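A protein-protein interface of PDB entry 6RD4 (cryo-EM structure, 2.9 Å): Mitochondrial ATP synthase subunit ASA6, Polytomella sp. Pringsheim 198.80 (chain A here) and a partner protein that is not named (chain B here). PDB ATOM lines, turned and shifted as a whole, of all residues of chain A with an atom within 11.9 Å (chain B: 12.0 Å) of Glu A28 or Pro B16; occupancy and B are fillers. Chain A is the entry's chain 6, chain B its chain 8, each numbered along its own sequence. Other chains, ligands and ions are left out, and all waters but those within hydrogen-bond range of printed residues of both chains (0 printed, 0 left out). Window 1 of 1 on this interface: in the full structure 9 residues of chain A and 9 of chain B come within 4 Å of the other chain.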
ATOM      1  N   GLU A  28     -30.026  27.986 -25.081  1.00  0.00           N
ATOM      2  CA  GLU A  28     -29.665  28.669 -23.848  1.00  0.00           C
ATOM      3  C   GLU A  28     -28.189  29.035 -23.850  1.00  0.00           C
ATOM      4  O   GLU A  28     -27.336  28.201 -23.557  1.00  0.00           O
ATOM      5  CB  GLU A  28     -29.991  27.794 -22.645  1.00  0.00           C
ATOM      6  CG  GLU A  28     -29.777  28.468 -21.311  1.00  0.00           C
ATOM      7  CD  GLU A  28     -30.060  27.551 -20.148  1.00  0.00           C
ATOM      8  OE1 GLU A  28     -30.166  26.332 -20.366  1.00  0.00           O
ATOM      9  OE2 GLU A  28     -30.180  28.051 -19.019  1.00  0.00           O
ATOM     10  N   GLY A  29     -27.889  30.279 -24.201  1.00  0.00           N
ATOM     11  CA  GLY A  29     -26.523  30.748 -24.188  1.00  0.00           C
ATOM     12  C   GLY A  29     -26.039  30.954 -22.779  1.00  0.00           C
ATOM     13  O   GLY A  29     -26.805  30.913 -21.817  1.00  0.00           O
ATOM     14  N   ASN A  30     -24.741  31.176 -22.641  1.00  0.00           N
ATOM     15  CA  ASN A  30     -24.189  31.156 -21.305  1.00  0.00           C
ATOM     16  C   ASN A  30     -24.409  32.483 -20.617  1.00  0.00           C
ATOM     17  O   ASN A  30     -24.495  33.524 -21.253  1.00  0.00           O
ATOM     18  CB  ASN A  30     -22.714  30.766 -21.318  1.00  0.00           C
ATOM     19  CG  ASN A  30     -21.831  31.854 -21.733  1.00  0.00           C
ATOM     20  OD1 ASN A  30     -22.098  32.511 -22.701  1.00  0.00           O
ATOM     21  ND2 ASN A  30     -20.736  32.018 -21.039  1.00  0.00           N
ATOM     22  N   SER A  31     -24.529  32.427 -19.302  1.00  0.00           N
ATOM     23  CA  SER A  31     -25.010  33.552 -18.532  1.00  0.00           C
ATOM     24  C   SER A  31     -23.962  34.610 -18.318  1.00  0.00           C
ATOM     25  O   SER A  31     -24.301  35.714 -17.911  1.00  0.00           O
ATOM     26  CB  SER A  31     -25.498  33.085 -17.182  1.00  0.00           C
ATOM     27  OG  SER A  31     -24.418  32.665 -16.395  1.00  0.00           O
ATOM     28  N   VAL A  32     -22.699  34.302 -18.547  1.00  0.00           N
ATOM     29  CA  VAL A  32     -21.684  35.332 -18.442  1.00  0.00           C
ATOM     30  C   VAL A  32     -21.714  36.226 -19.665  1.00  0.00           C
ATOM     31  O   VAL A  32     -21.607  37.444 -19.549  1.00  0.00           O
ATOM     32  CB  VAL A  32     -20.318  34.682 -18.212  1.00  0.00           C
ATOM     33  CG1 VAL A  32     -19.268  35.701 -18.169  1.00  0.00           C
ATOM     34  CG2 VAL A  32     -20.345  33.998 -16.911  1.00  0.00           C
ATOM     35  N   ALA A  33     -21.924  35.663 -20.849  1.00  0.00           N
ATOM     36  CA  ALA A  33     -22.165  36.500 -22.011  1.00  0.00           C
ATOM     37  C   ALA A  33     -23.488  37.236 -21.923  1.00  0.00           C
ATOM     38  O   ALA A  33     -23.668  38.243 -22.607  1.00  0.00           O
ATOM     39  CB  ALA A  33     -22.140  35.685 -23.289  1.00  0.00           C
ATOM     40  N   GLY A  34     -24.423  36.752 -21.116  1.00  0.00           N
ATOM     41  CA  GLY A  34     -25.597  37.538 -20.822  1.00  0.00           C
ATOM     42  C   GLY A  34     -25.329  38.639 -19.828  1.00  0.00           C
ATOM     43  O   GLY A  34     -25.993  39.667 -19.856  1.00  0.00           O
ATOM     44  N   ILE A  35     -24.376  38.432 -18.923  1.00  0.00           N
ATOM     45  CA  ILE A  35     -23.976  39.485 -17.997  1.00  0.00           C
ATOM     46  C   ILE A  35     -23.205  40.557 -18.737  1.00  0.00           C
ATOM     47  O   ILE A  35     -23.449  41.749 -18.554  1.00  0.00           O
ATOM     48  CB  ILE A  35     -23.148  38.889 -16.845  1.00  0.00           C
ATOM     49  CG1 ILE A  35     -24.053  38.300 -15.788  1.00  0.00           C
ATOM     50  CG2 ILE A  35     -22.280  39.906 -16.185  1.00  0.00           C
ATOM     51  CD1 ILE A  35     -23.319  37.604 -14.693  1.00  0.00           C
ATOM     52  N   LYS A  37     -23.302  41.312 -21.899  1.00  0.00           N
ATOM     53  CA  LYS A  37     -24.154  42.078 -22.795  1.00  0.00           C
ATOM     54  C   LYS A  37     -25.053  43.026 -22.024  1.00  0.00           C
ATOM     55  O   LYS A  37     -25.179  44.184 -22.396  1.00  0.00           O
ATOM     56  CB  LYS A  37     -24.981  41.153 -23.669  1.00  0.00           C
ATOM     57  CG  LYS A  37     -25.234  41.709 -25.048  1.00  0.00           C
ATOM     58  CD  LYS A  37     -26.112  40.806 -25.871  1.00  0.00           C
ATOM     59  CE  LYS A  37     -27.481  40.689 -25.259  1.00  0.00           C
ATOM     60  NZ  LYS A  37     -28.156  41.999 -25.162  1.00  0.00           N
ATOM     61  N   LYS A  55     -27.845  40.463 -11.918  1.00  0.00           N
ATOM     62  CA  LYS A  55     -27.443  39.384 -11.031  1.00  0.00           C
ATOM     63  C   LYS A  55     -28.458  38.260 -11.052  1.00  0.00           C
ATOM     64  O   LYS A  55     -28.089  37.085 -11.100  1.00  0.00           O
ATOM     65  CB  LYS A  55     -27.291  39.913  -9.614  1.00  0.00           C
ATOM     66  CG  LYS A  55     -26.933  38.908  -8.576  1.00  0.00           C
ATOM     67  CD  LYS A  55     -25.462  38.673  -8.550  1.00  0.00           C
ATOM     68  CE  LYS A  55     -25.058  37.937  -7.308  1.00  0.00           C
ATOM     69  NZ  LYS A  55     -23.619  37.588  -7.341  1.00  0.00           N
ATOM     70  N   ALA A  56     -29.737  38.601 -11.028  1.00  0.00           N
ATOM     71  CA  ALA A  56     -30.799  37.616 -10.964  1.00  0.00           C
ATOM     72  C   ALA A  56     -31.197  37.081 -12.323  1.00  0.00           C
ATOM     73  O   ALA A  56     -31.875  36.063 -12.387  1.00  0.00           O
ATOM     74  CB  ALA A  56     -32.015  38.219 -10.281  1.00  0.00           C
ATOM     75  N   GLN A  57     -30.823  37.746 -13.404  1.00  0.00           N
ATOM     76  CA  GLN A  57     -31.045  37.178 -14.721  1.00  0.00           C
ATOM     77  C   GLN A  57     -30.030  36.109 -15.059  1.00  0.00           C
ATOM     78  O   GLN A  57     -30.237  35.351 -16.008  1.00  0.00           O
ATOM     79  CB  GLN A  57     -30.979  38.261 -15.784  1.00  0.00           C
ATOM     80  CG  GLN A  57     -32.305  38.805 -16.200  1.00  0.00           C
ATOM     81  CD  GLN A  57     -32.168  40.016 -17.092  1.00  0.00           C
ATOM     82  OE1 GLN A  57     -31.093  40.596 -17.206  1.00  0.00           O
ATOM     83  NE2 GLN A  57     -33.263  40.410 -17.727  1.00  0.00           N
ATOM     84  N   ALA A  58     -28.928  36.052 -14.323  1.00  0.00           N
ATOM     85  CA  ALA A  58     -27.869  35.089 -14.556  1.00  0.00           C
ATOM     86  C   ALA A  58     -27.672  34.160 -13.379  1.00  0.00           C
ATOM     87  O   ALA A  58     -26.678  33.438 -13.339  1.00  0.00           O
ATOM     88  CB  ALA A  58     -26.563  35.802 -14.854  1.00  0.00           C
ATOM     89  N   ALA A  59     -28.567  34.191 -12.409  1.00  0.00           N
ATOM     90  CA  ALA A  59     -28.578  33.189 -11.376  1.00  0.00           C
ATOM     91  C   ALA A  59     -29.029  31.868 -11.978  1.00  0.00           C
ATOM     92  O   ALA A  59     -29.785  31.858 -12.945  1.00  0.00           O
ATOM     93  CB  ALA A  59     -29.516  33.606 -10.257  1.00  0.00           C
ATOM     94  N   PRO A  60     -28.556  30.740 -11.458  1.00  0.00           N
ATOM     95  CA  PRO A  60     -29.004  29.457 -11.988  1.00  0.00           C
ATOM     96  C   PRO A  60     -30.415  29.146 -11.536  1.00  0.00           C
ATOM     97  O   PRO A  60     -30.898  29.648 -10.523  1.00  0.00           O
ATOM     98  CB  PRO A  60     -28.003  28.473 -11.403  1.00  0.00           C
ATOM     99  CG  PRO A  60     -27.562  29.102 -10.200  1.00  0.00           C
ATOM    100  CD  PRO A  60     -27.501  30.546 -10.456  1.00  0.00           C
ATOM    101  N   ILE A  61     -31.089  28.311 -12.310  1.00  0.00           N
ATOM    102  CA  ILE A  61     -32.447  27.924 -11.958  1.00  0.00           C
ATOM    103  C   ILE A  61     -32.384  26.888 -10.850  1.00  0.00           C
ATOM    104  O   ILE A  61     -31.624  25.922 -10.918  1.00  0.00           O
ATOM    105  CB  ILE A  61     -33.227  27.425 -13.187  1.00  0.00           C
ATOM    106  CG1 ILE A  61     -34.636  27.022 -12.801  1.00  0.00           C
ATOM    107  CG2 ILE A  61     -32.561  26.275 -13.898  1.00  0.00           C
ATOM    108  CD1 ILE A  61     -35.479  28.164 -12.408  1.00  0.00           C
ATOM    109  N   TYR A  62     -33.092  27.149  -9.778  1.00  0.00           N
ATOM    110  CA  TYR A  62     -33.350  26.142  -8.767  1.00  0.00           C
ATOM    111  C   TYR A  62     -34.846  25.960  -8.784  1.00  0.00           C
ATOM    112  O   TYR A  62     -35.566  26.850  -8.296  1.00  0.00           O
ATOM    113  CB  TYR A  62     -32.878  26.599  -7.399  1.00  0.00           C
ATOM    114  CG  TYR A  62     -31.424  26.939  -7.338  1.00  0.00           C
ATOM    115  CD1 TYR A  62     -30.484  26.130  -7.915  1.00  0.00           C
ATOM    116  CD2 TYR A  62     -30.993  28.074  -6.696  1.00  0.00           C
ATOM    117  CE1 TYR A  62     -29.168  26.438  -7.854  1.00  0.00           C
ATOM    118  CE2 TYR A  62     -29.676  28.384  -6.637  1.00  0.00           C
ATOM    119  CZ  TYR A  62     -28.771  27.557  -7.217  1.00  0.00           C
ATOM    120  OH  TYR A  62     -27.449  27.867  -7.154  1.00  0.00           O
ATOM    121  N   PRO A  63     -35.354  24.866  -9.347  1.00  0.00           N
ATOM    122  CA  PRO A  63     -36.786  24.749  -9.606  1.00  0.00           C
ATOM    123  C   PRO A  63     -37.610  24.728  -8.337  1.00  0.00           C
ATOM    124  O   PRO A  63     -37.162  24.263  -7.291  1.00  0.00           O
ATOM    125  CB  PRO A  63     -36.885  23.428 -10.361  1.00  0.00           C
ATOM    126  CG  PRO A  63     -35.595  23.289 -10.985  1.00  0.00           C
ATOM    127  CD  PRO A  63     -34.618  23.793 -10.012  1.00  0.00           C
ATOM    128  N   ALA A  64     -38.788  25.324  -8.421  1.00  0.00           N
ATOM    129  CA  ALA A  64     -39.564  25.591  -7.232  1.00  0.00           C
ATOM    130  C   ALA A  64     -40.325  24.352  -6.804  1.00  0.00           C
ATOM    131  O   ALA A  64     -40.652  23.482  -7.612  1.00  0.00           O
ATOM    132  CB  ALA A  64     -40.525  26.749  -7.470  1.00  0.00           C
ATOM    133  N   GLY B   4     -15.701  35.288 -27.928  1.00  0.00           N
ATOM    134  CA  GLY B   4     -17.094  35.625 -28.063  1.00  0.00           C
ATOM    135  C   GLY B   4     -18.119  34.529 -28.185  1.00  0.00           C
ATOM    136  O   GLY B   4     -18.929  34.587 -29.114  1.00  0.00           O
ATOM    137  N   GLU B   5     -18.024  33.483 -27.367  1.00  0.00           N
ATOM    138  CA  GLU B   5     -19.064  32.476 -27.141  1.00  0.00           C
ATOM    139  C   GLU B   5     -19.260  31.519 -28.303  1.00  0.00           C
ATOM    140  O   GLU B   5     -19.942  30.506 -28.162  1.00  0.00           O
ATOM    141  CB  GLU B   5     -20.409  33.115 -26.792  1.00  0.00           C
ATOM    142  CG  GLU B   5     -21.250  32.299 -25.870  1.00  0.00           C
ATOM    143  CD  GLU B   5     -22.711  32.606 -26.029  1.00  0.00           C
ATOM    144  OE1 GLU B   5     -23.036  33.739 -26.429  1.00  0.00           O
ATOM    145  OE2 GLU B   5     -23.541  31.710 -25.775  1.00  0.00           O
ATOM    146  N   VAL B   6     -18.650  31.780 -29.444  1.00  0.00           N
ATOM    147  CA  VAL B   6     -18.566  30.740 -30.446  1.00  0.00           C
ATOM    148  C   VAL B   6     -17.367  29.860 -30.145  1.00  0.00           C
ATOM    149  O   VAL B   6     -17.291  28.730 -30.639  1.00  0.00           O
ATOM    150  CB  VAL B   6     -18.519  31.358 -31.853  1.00  0.00           C
ATOM    151  CG1 VAL B   6     -17.164  31.919 -32.157  1.00  0.00           C
ATOM    152  CG2 VAL B   6     -18.958  30.371 -32.903  1.00  0.00           C
ATOM    153  N   LEU B   8     -16.574  29.067 -26.890  1.00  0.00           N
ATOM    154  CA  LEU B   8     -16.997  28.283 -25.749  1.00  0.00           C
ATOM    155  C   LEU B   8     -18.132  27.338 -26.071  1.00  0.00           C
ATOM    156  O   LEU B   8     -18.674  26.731 -25.154  1.00  0.00           O
ATOM    157  CB  LEU B   8     -17.462  29.189 -24.624  1.00  0.00           C
ATOM    158  CG  LEU B   8     -16.612  30.230 -23.950  1.00  0.00           C
ATOM    159  CD1 LEU B   8     -17.566  30.930 -23.129  1.00  0.00           C
ATOM    160  CD2 LEU B   8     -15.655  29.602 -23.059  1.00  0.00           C
ATOM    161  N   LYS B   9     -18.543  27.226 -27.322  1.00  0.00           N
ATOM    162  CA  LYS B   9     -19.715  26.431 -27.645  1.00  0.00           C
ATOM    163  C   LYS B   9     -19.392  24.954 -27.570  1.00  0.00           C
ATOM    164  O   LYS B   9     -18.430  24.494 -28.186  1.00  0.00           O
ATOM    165  CB  LYS B   9     -20.229  26.769 -29.033  1.00  0.00           C
ATOM    166  CG  LYS B   9     -21.583  26.197 -29.316  1.00  0.00           C
ATOM    167  CD  LYS B   9     -21.942  26.341 -30.759  1.00  0.00           C
ATOM    168  CE  LYS B   9     -21.247  25.301 -31.604  1.00  0.00           C
ATOM    169  NZ  LYS B   9     -21.954  24.002 -31.581  1.00  0.00           N
ATOM    170  N   ASP B  10     -20.202  24.232 -26.792  1.00  0.00           N
ATOM    171  CA  ASP B  10     -20.109  22.793 -26.560  1.00  0.00           C
ATOM    172  C   ASP B  10     -18.797  22.401 -25.910  1.00  0.00           C
ATOM    173  O   ASP B  10     -18.331  21.281 -26.073  1.00  0.00           O
ATOM    174  CB  ASP B  10     -20.333  21.997 -27.838  1.00  0.00           C
ATOM    175  CG  ASP B  10     -21.691  22.235 -28.433  1.00  0.00           C
ATOM    176  OD1 ASP B  10     -22.617  22.574 -27.675  1.00  0.00           O
ATOM    177  OD2 ASP B  10     -21.843  22.074 -29.656  1.00  0.00           O
ATOM    178  N   ILE B  11     -18.199  23.317 -25.169  1.00  0.00           N
ATOM    179  CA  ILE B  11     -16.944  23.084 -24.486  1.00  0.00           C
ATOM    180  C   ILE B  11     -17.165  23.421 -23.029  1.00  0.00           C
ATOM    181  O   ILE B  11     -16.945  22.592 -22.145  1.00  0.00           O
ATOM    182  CB  ILE B  11     -15.808  23.920 -25.080  1.00  0.00           C
ATOM    183  CG1 ILE B  11     -15.445  23.414 -26.461  1.00  0.00           C
ATOM    184  CG2 ILE B  11     -14.622  23.804 -24.238  1.00  0.00           C
ATOM    185  CD1 ILE B  11     -14.501  24.275 -27.184  1.00  0.00           C
ATOM    186  N   LEU B  12     -17.613  24.641 -22.772  1.00  0.00           N
ATOM    187  CA  LEU B  12     -17.835  25.138 -21.428  1.00  0.00           C
ATOM    188  C   LEU B  12     -19.174  25.826 -21.396  1.00  0.00           C
ATOM    189  O   LEU B  12     -19.384  26.790 -22.126  1.00  0.00           O
ATOM    190  CB  LEU B  12     -16.761  26.129 -21.015  1.00  0.00           C
ATOM    191  CG  LEU B  12     -15.371  25.645 -20.684  1.00  0.00           C
ATOM    192  CD1 LEU B  12     -14.512  26.830 -20.780  1.00  0.00           C
ATOM    193  CD2 LEU B  12     -15.352  25.117 -19.305  1.00  0.00           C
ATOM    194  N   ARG B  13     -20.070  25.353 -20.555  1.00  0.00           N
ATOM    195  CA  ARG B  13     -21.340  26.014 -20.364  1.00  0.00           C
ATOM    196  C   ARG B  13     -21.447  26.460 -18.921  1.00  0.00           C
ATOM    197  O   ARG B  13     -20.756  25.949 -18.051  1.00  0.00           O
ATOM    198  CB  ARG B  13     -22.479  25.106 -20.728  1.00  0.00           C
ATOM    199  CG  ARG B  13     -22.281  24.423 -22.025  1.00  0.00           C
ATOM    200  CD  ARG B  13     -23.560  23.922 -22.538  1.00  0.00           C
ATOM    201  NE  ARG B  13     -23.387  23.270 -23.815  1.00  0.00           N
ATOM    202  CZ  ARG B  13     -23.352  21.964 -23.981  1.00  0.00           C
ATOM    203  NH1 ARG B  13     -23.200  21.455 -25.180  1.00  0.00           N
ATOM    204  NH2 ARG B  13     -23.484  21.174 -22.951  1.00  0.00           N
ATOM    205  N   THR B  14     -22.282  27.450 -18.683  1.00  0.00           N
ATOM    206  CA  THR B  14     -22.521  27.970 -17.349  1.00  0.00           C
ATOM    207  C   THR B  14     -23.640  27.168 -16.706  1.00  0.00           C
ATOM    208  O   THR B  14     -24.255  26.348 -17.381  1.00  0.00           O
ATOM    209  CB  THR B  14     -22.867  29.443 -17.462  1.00  0.00           C
ATOM    210  OG1 THR B  14     -23.877  29.583 -18.450  1.00  0.00           O
ATOM    211  CG2 THR B  14     -21.651  30.229 -17.840  1.00  0.00           C
ATOM    212  N   PRO B  15     -23.900  27.337 -15.407  1.00  0.00           N
ATOM    213  CA  PRO B  15     -25.049  26.682 -14.797  1.00  0.00           C
ATOM    214  C   PRO B  15     -26.345  27.115 -15.440  1.00  0.00           C
ATOM    215  O   PRO B  15     -26.498  28.293 -15.787  1.00  0.00           O
ATOM    216  CB  PRO B  15     -24.985  27.140 -13.340  1.00  0.00           C
ATOM    217  CG  PRO B  15     -23.939  28.119 -13.290  1.00  0.00           C
ATOM    218  CD  PRO B  15     -23.001  27.786 -14.343  1.00  0.00           C
ATOM    219  N   PRO B  16     -27.279  26.191 -15.647  1.00  0.00           N
ATOM    220  CA  PRO B  16     -28.453  26.502 -16.456  1.00  0.00           C
ATOM    221  C   PRO B  16     -29.391  27.462 -15.761  1.00  0.00           C
ATOM    222  O   PRO B  16     -29.553  27.440 -14.545  1.00  0.00           O
ATOM    223  CB  PRO B  16     -29.103  25.134 -16.666  1.00  0.00           C
ATOM    224  CG  PRO B  16     -28.578  24.296 -15.615  1.00  0.00           C
ATOM    225  CD  PRO B  16     -27.215  24.761 -15.325  1.00  0.00           C
ATOM    226  N   THR B  17     -29.982  28.340 -16.559  1.00  0.00           N
ATOM    227  CA  THR B  17     -30.924  29.341 -16.090  1.00  0.00           C
ATOM    228  C   THR B  17     -32.345  29.053 -16.522  1.00  0.00           C
ATOM    229  O   THR B  17     -33.279  29.434 -15.821  1.00  0.00           O
ATOM    230  CB  THR B  17     -30.532  30.723 -16.614  1.00  0.00           C
ATOM    231  OG1 THR B  17     -30.476  30.677 -18.039  1.00  0.00           O
ATOM    232  CG2 THR B  17     -29.184  31.121 -16.114  1.00  0.00           C
ATOM    233  N   GLY B  18     -32.527  28.396 -17.655  1.00  0.00           N
ATOM    234  CA  GLY B  18     -33.857  28.102 -18.123  1.00  0.00           C
ATOM    235  C   GLY B  18     -34.469  26.952 -17.376  1.00  0.00           C
ATOM    236  O   GLY B  18     -35.401  27.139 -16.594  1.00  0.00           O
ATOM    237  N   ALA B  19     -33.941  25.756 -17.592  1.00  0.00           N
ATOM    238  CA  ALA B  19     -34.439  24.584 -16.899  1.00  0.00           C
ATOM    239  C   ALA B  19     -33.317  23.573 -16.821  1.00  0.00           C
ATOM    240  O   ALA B  19     -32.377  23.615 -17.612  1.00  0.00           O
ATOM    241  CB  ALA B  19     -35.655  23.987 -17.603  1.00  0.00           C
ATOM    242  N   ILE B  20     -33.422  22.676 -15.856  1.00  0.00           N
ATOM    243  CA  ILE B  20     -32.415  21.632 -15.681  1.00  0.00           C
ATOM    244  C   ILE B  20     -32.553  20.621 -16.808  1.00  0.00           C
ATOM    245  O   ILE B  20     -33.657  20.112 -17.038  1.00  0.00           O
ATOM    246  CB  ILE B  20     -32.580  20.976 -14.329  1.00  0.00           C
ATOM    247  CG1 ILE B  20     -32.328  22.014 -13.269  1.00  0.00           C
ATOM    248  CG2 ILE B  20     -31.598  19.890 -14.147  1.00  0.00           C
ATOM    249  CD1 ILE B  20     -32.485  21.511 -11.933  1.00  0.00           C
ATOM    250  N   PRO B  21     -31.494  20.310 -17.537  1.00  0.00           N
ATOM    251  CA  PRO B  21     -31.623  19.471 -18.721  1.00  0.00           C
ATOM    252  C   PRO B  21     -31.795  18.009 -18.342  1.00  0.00           C
ATOM    253  O   PRO B  21     -31.844  17.637 -17.179  1.00  0.00           O
ATOM    254  CB  PRO B  21     -30.304  19.695 -19.450  1.00  0.00           C
ATOM    255  CG  PRO B  21     -29.619  20.739 -18.727  1.00  0.00           C
ATOM    256  CD  PRO B  21     -30.115  20.772 -17.369  1.00  0.00           C
ATOM    257  N   ALA B  22     -31.894  17.174 -19.357  1.00  0.00           N
ATOM    258  CA  ALA B  22     -31.869  15.752 -19.118  1.00  0.00           C
ATOM    259  C   ALA B  22     -30.443  15.307 -18.855  1.00  0.00           C
ATOM    260  O   ALA B  22     -29.487  15.913 -19.338  1.00  0.00           O
ATOM    261  CB  ALA B  22     -32.443  15.009 -20.311  1.00  0.00           C
ATOM    262  N   ASN B  23     -30.303  14.250 -18.067  1.00  0.00           N
ATOM    263  CA  ASN B  23     -28.994  13.673 -17.827  1.00  0.00           C
ATOM    264  C   ASN B  23     -28.480  13.038 -19.103  1.00  0.00           C
ATOM    265  O   ASN B  23     -29.251  12.507 -19.901  1.00  0.00           O
ATOM    266  CB  ASN B  23     -29.082  12.650 -16.710  1.00  0.00           C
ATOM    267  CG  ASN B  23     -27.753  12.311 -16.134  1.00  0.00           C
ATOM    268  OD1 ASN B  23     -26.736  12.818 -16.565  1.00  0.00           O
ATOM    269  ND2 ASN B  23     -27.752  11.464 -15.129  1.00  0.00           N
ATOM    270  N   VAL B  24     -27.183  13.150 -19.326  1.00  0.00           N
ATOM    271  CA  VAL B  24     -26.560  12.542 -20.497  1.00  0.00           C
ATOM    272  C   VAL B  24     -26.400  11.049 -20.237  1.00  0.00           C
ATOM    273  O   VAL B  24     -25.809  10.670 -19.220  1.00  0.00           O
ATOM    274  CB  VAL B  24     -25.224  13.196 -20.784  1.00  0.00           C
ATOM    275  CG1 VAL B  24     -24.499  12.453 -21.830  1.00  0.00           C
ATOM    276  CG2 VAL B  24     -25.441  14.560 -21.236  1.00  0.00           C
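OG1 of Thr B14 is in hydrogen-bond range of N of Ser A31, 3.0 Å away. N of Gly B18 lies within hydrogen-bond range of OE2 of Glu A28, 2.7 Å away. The side-chain carboxylate (OE2) of Glu A28 is in hydrogen-bond range of the backbone NH (N) of Thr B17 (2.5 Å). OE2 of Glu B5 lies within hydrogen-bond range of N of Asn A30, at 3.4 Å. The backbone NH of Ile A61 lies within hydrogen-bond range of the backbone carbonyl oxygen of Pro B16 (2.8 Å).
Glu A28 touches Pro B16. Gly A29 touches Glu B5. Asn A30 touches Leu B8 (ND2 to CD1, 3.9 Å). Asn A30 touches Thr B14 (CA to OG1, 3.3 Å). Ala A33 touches Glu B5. Thr B17 touches Ala A59 (CG2 to O, 3.3 Å). Pro A60 touches Pro B15 (CB to CB, 3.8 Å). Thr B17 touches Ile A61 (O to CB, 3.3 Å). Ile A61 touches Gly B18 (CG1 to O, 3.9 Å). CG2 of Ile A61 touches CA of Ala B19, at 3.9 Å.
Glu A28 touches just these residues of chain B: Pro B16, Thr B17 and Gly B18. Pro B16 touches just these residues of chain A: Glu A28, Pro A60 and Ile A61. Of the printed residues of chain B, Ile A61 touches Pro B16 (2.8 Å), Thr B17 (3.3 Å), Gly B18 (3.9 Å) and Ala B19 (3.9 Å). Thr B14 touches just these residues of chain A: Asn A30 (3.3 Å) and Ser A31 (3.0 Å). Printed residues of chain A within 4 Å of Pro B15: Pro A60 (3.8 Å). Of chain A, only Glu A28, Ala A59 and Ile A61 come within 4 Å of Thr B17. Of chain A, only Glu A28 and Ile A61 come within 4 Å of Gly B18. Of chain A, only Ile A61 (3.9 Å) comes within 4 Å of Ala B19. No residue of chain A comes within 4 Å of Pro B21. Of the printed residues of chain B, Ala A33 touches Glu B5 (3.8 Å). Of the printed residues of chain B, Ser A31 touches Thr B14. Ala A64 touches none of the printed residues of chain B. Asn B23 touches none of the printed residues of chain A. The nearest printed residue of chain B that does not touch Pro A63 is Ala B19 (6.2 Å).
Printed residues of chain A that touch a printed residue of chain B: Glu A28, Gly A29, Asn A30, Ser A31, Ala A33, Ala A59, Pro A60, Ile A61 and Pro A63. Hydrophobic or aromatic side chains of chain A within 4 Å of the printed part of chain B: Ala A33, Pro A60, Ile A61 and Pro A63. Hydrophobic or aromatic side chains of chain B within 4 Å of the printed part of chain A: Leu B8, Pro B15, Pro B16 and Ile B20. Among the printed residues, 17 pairs touch across the chains.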
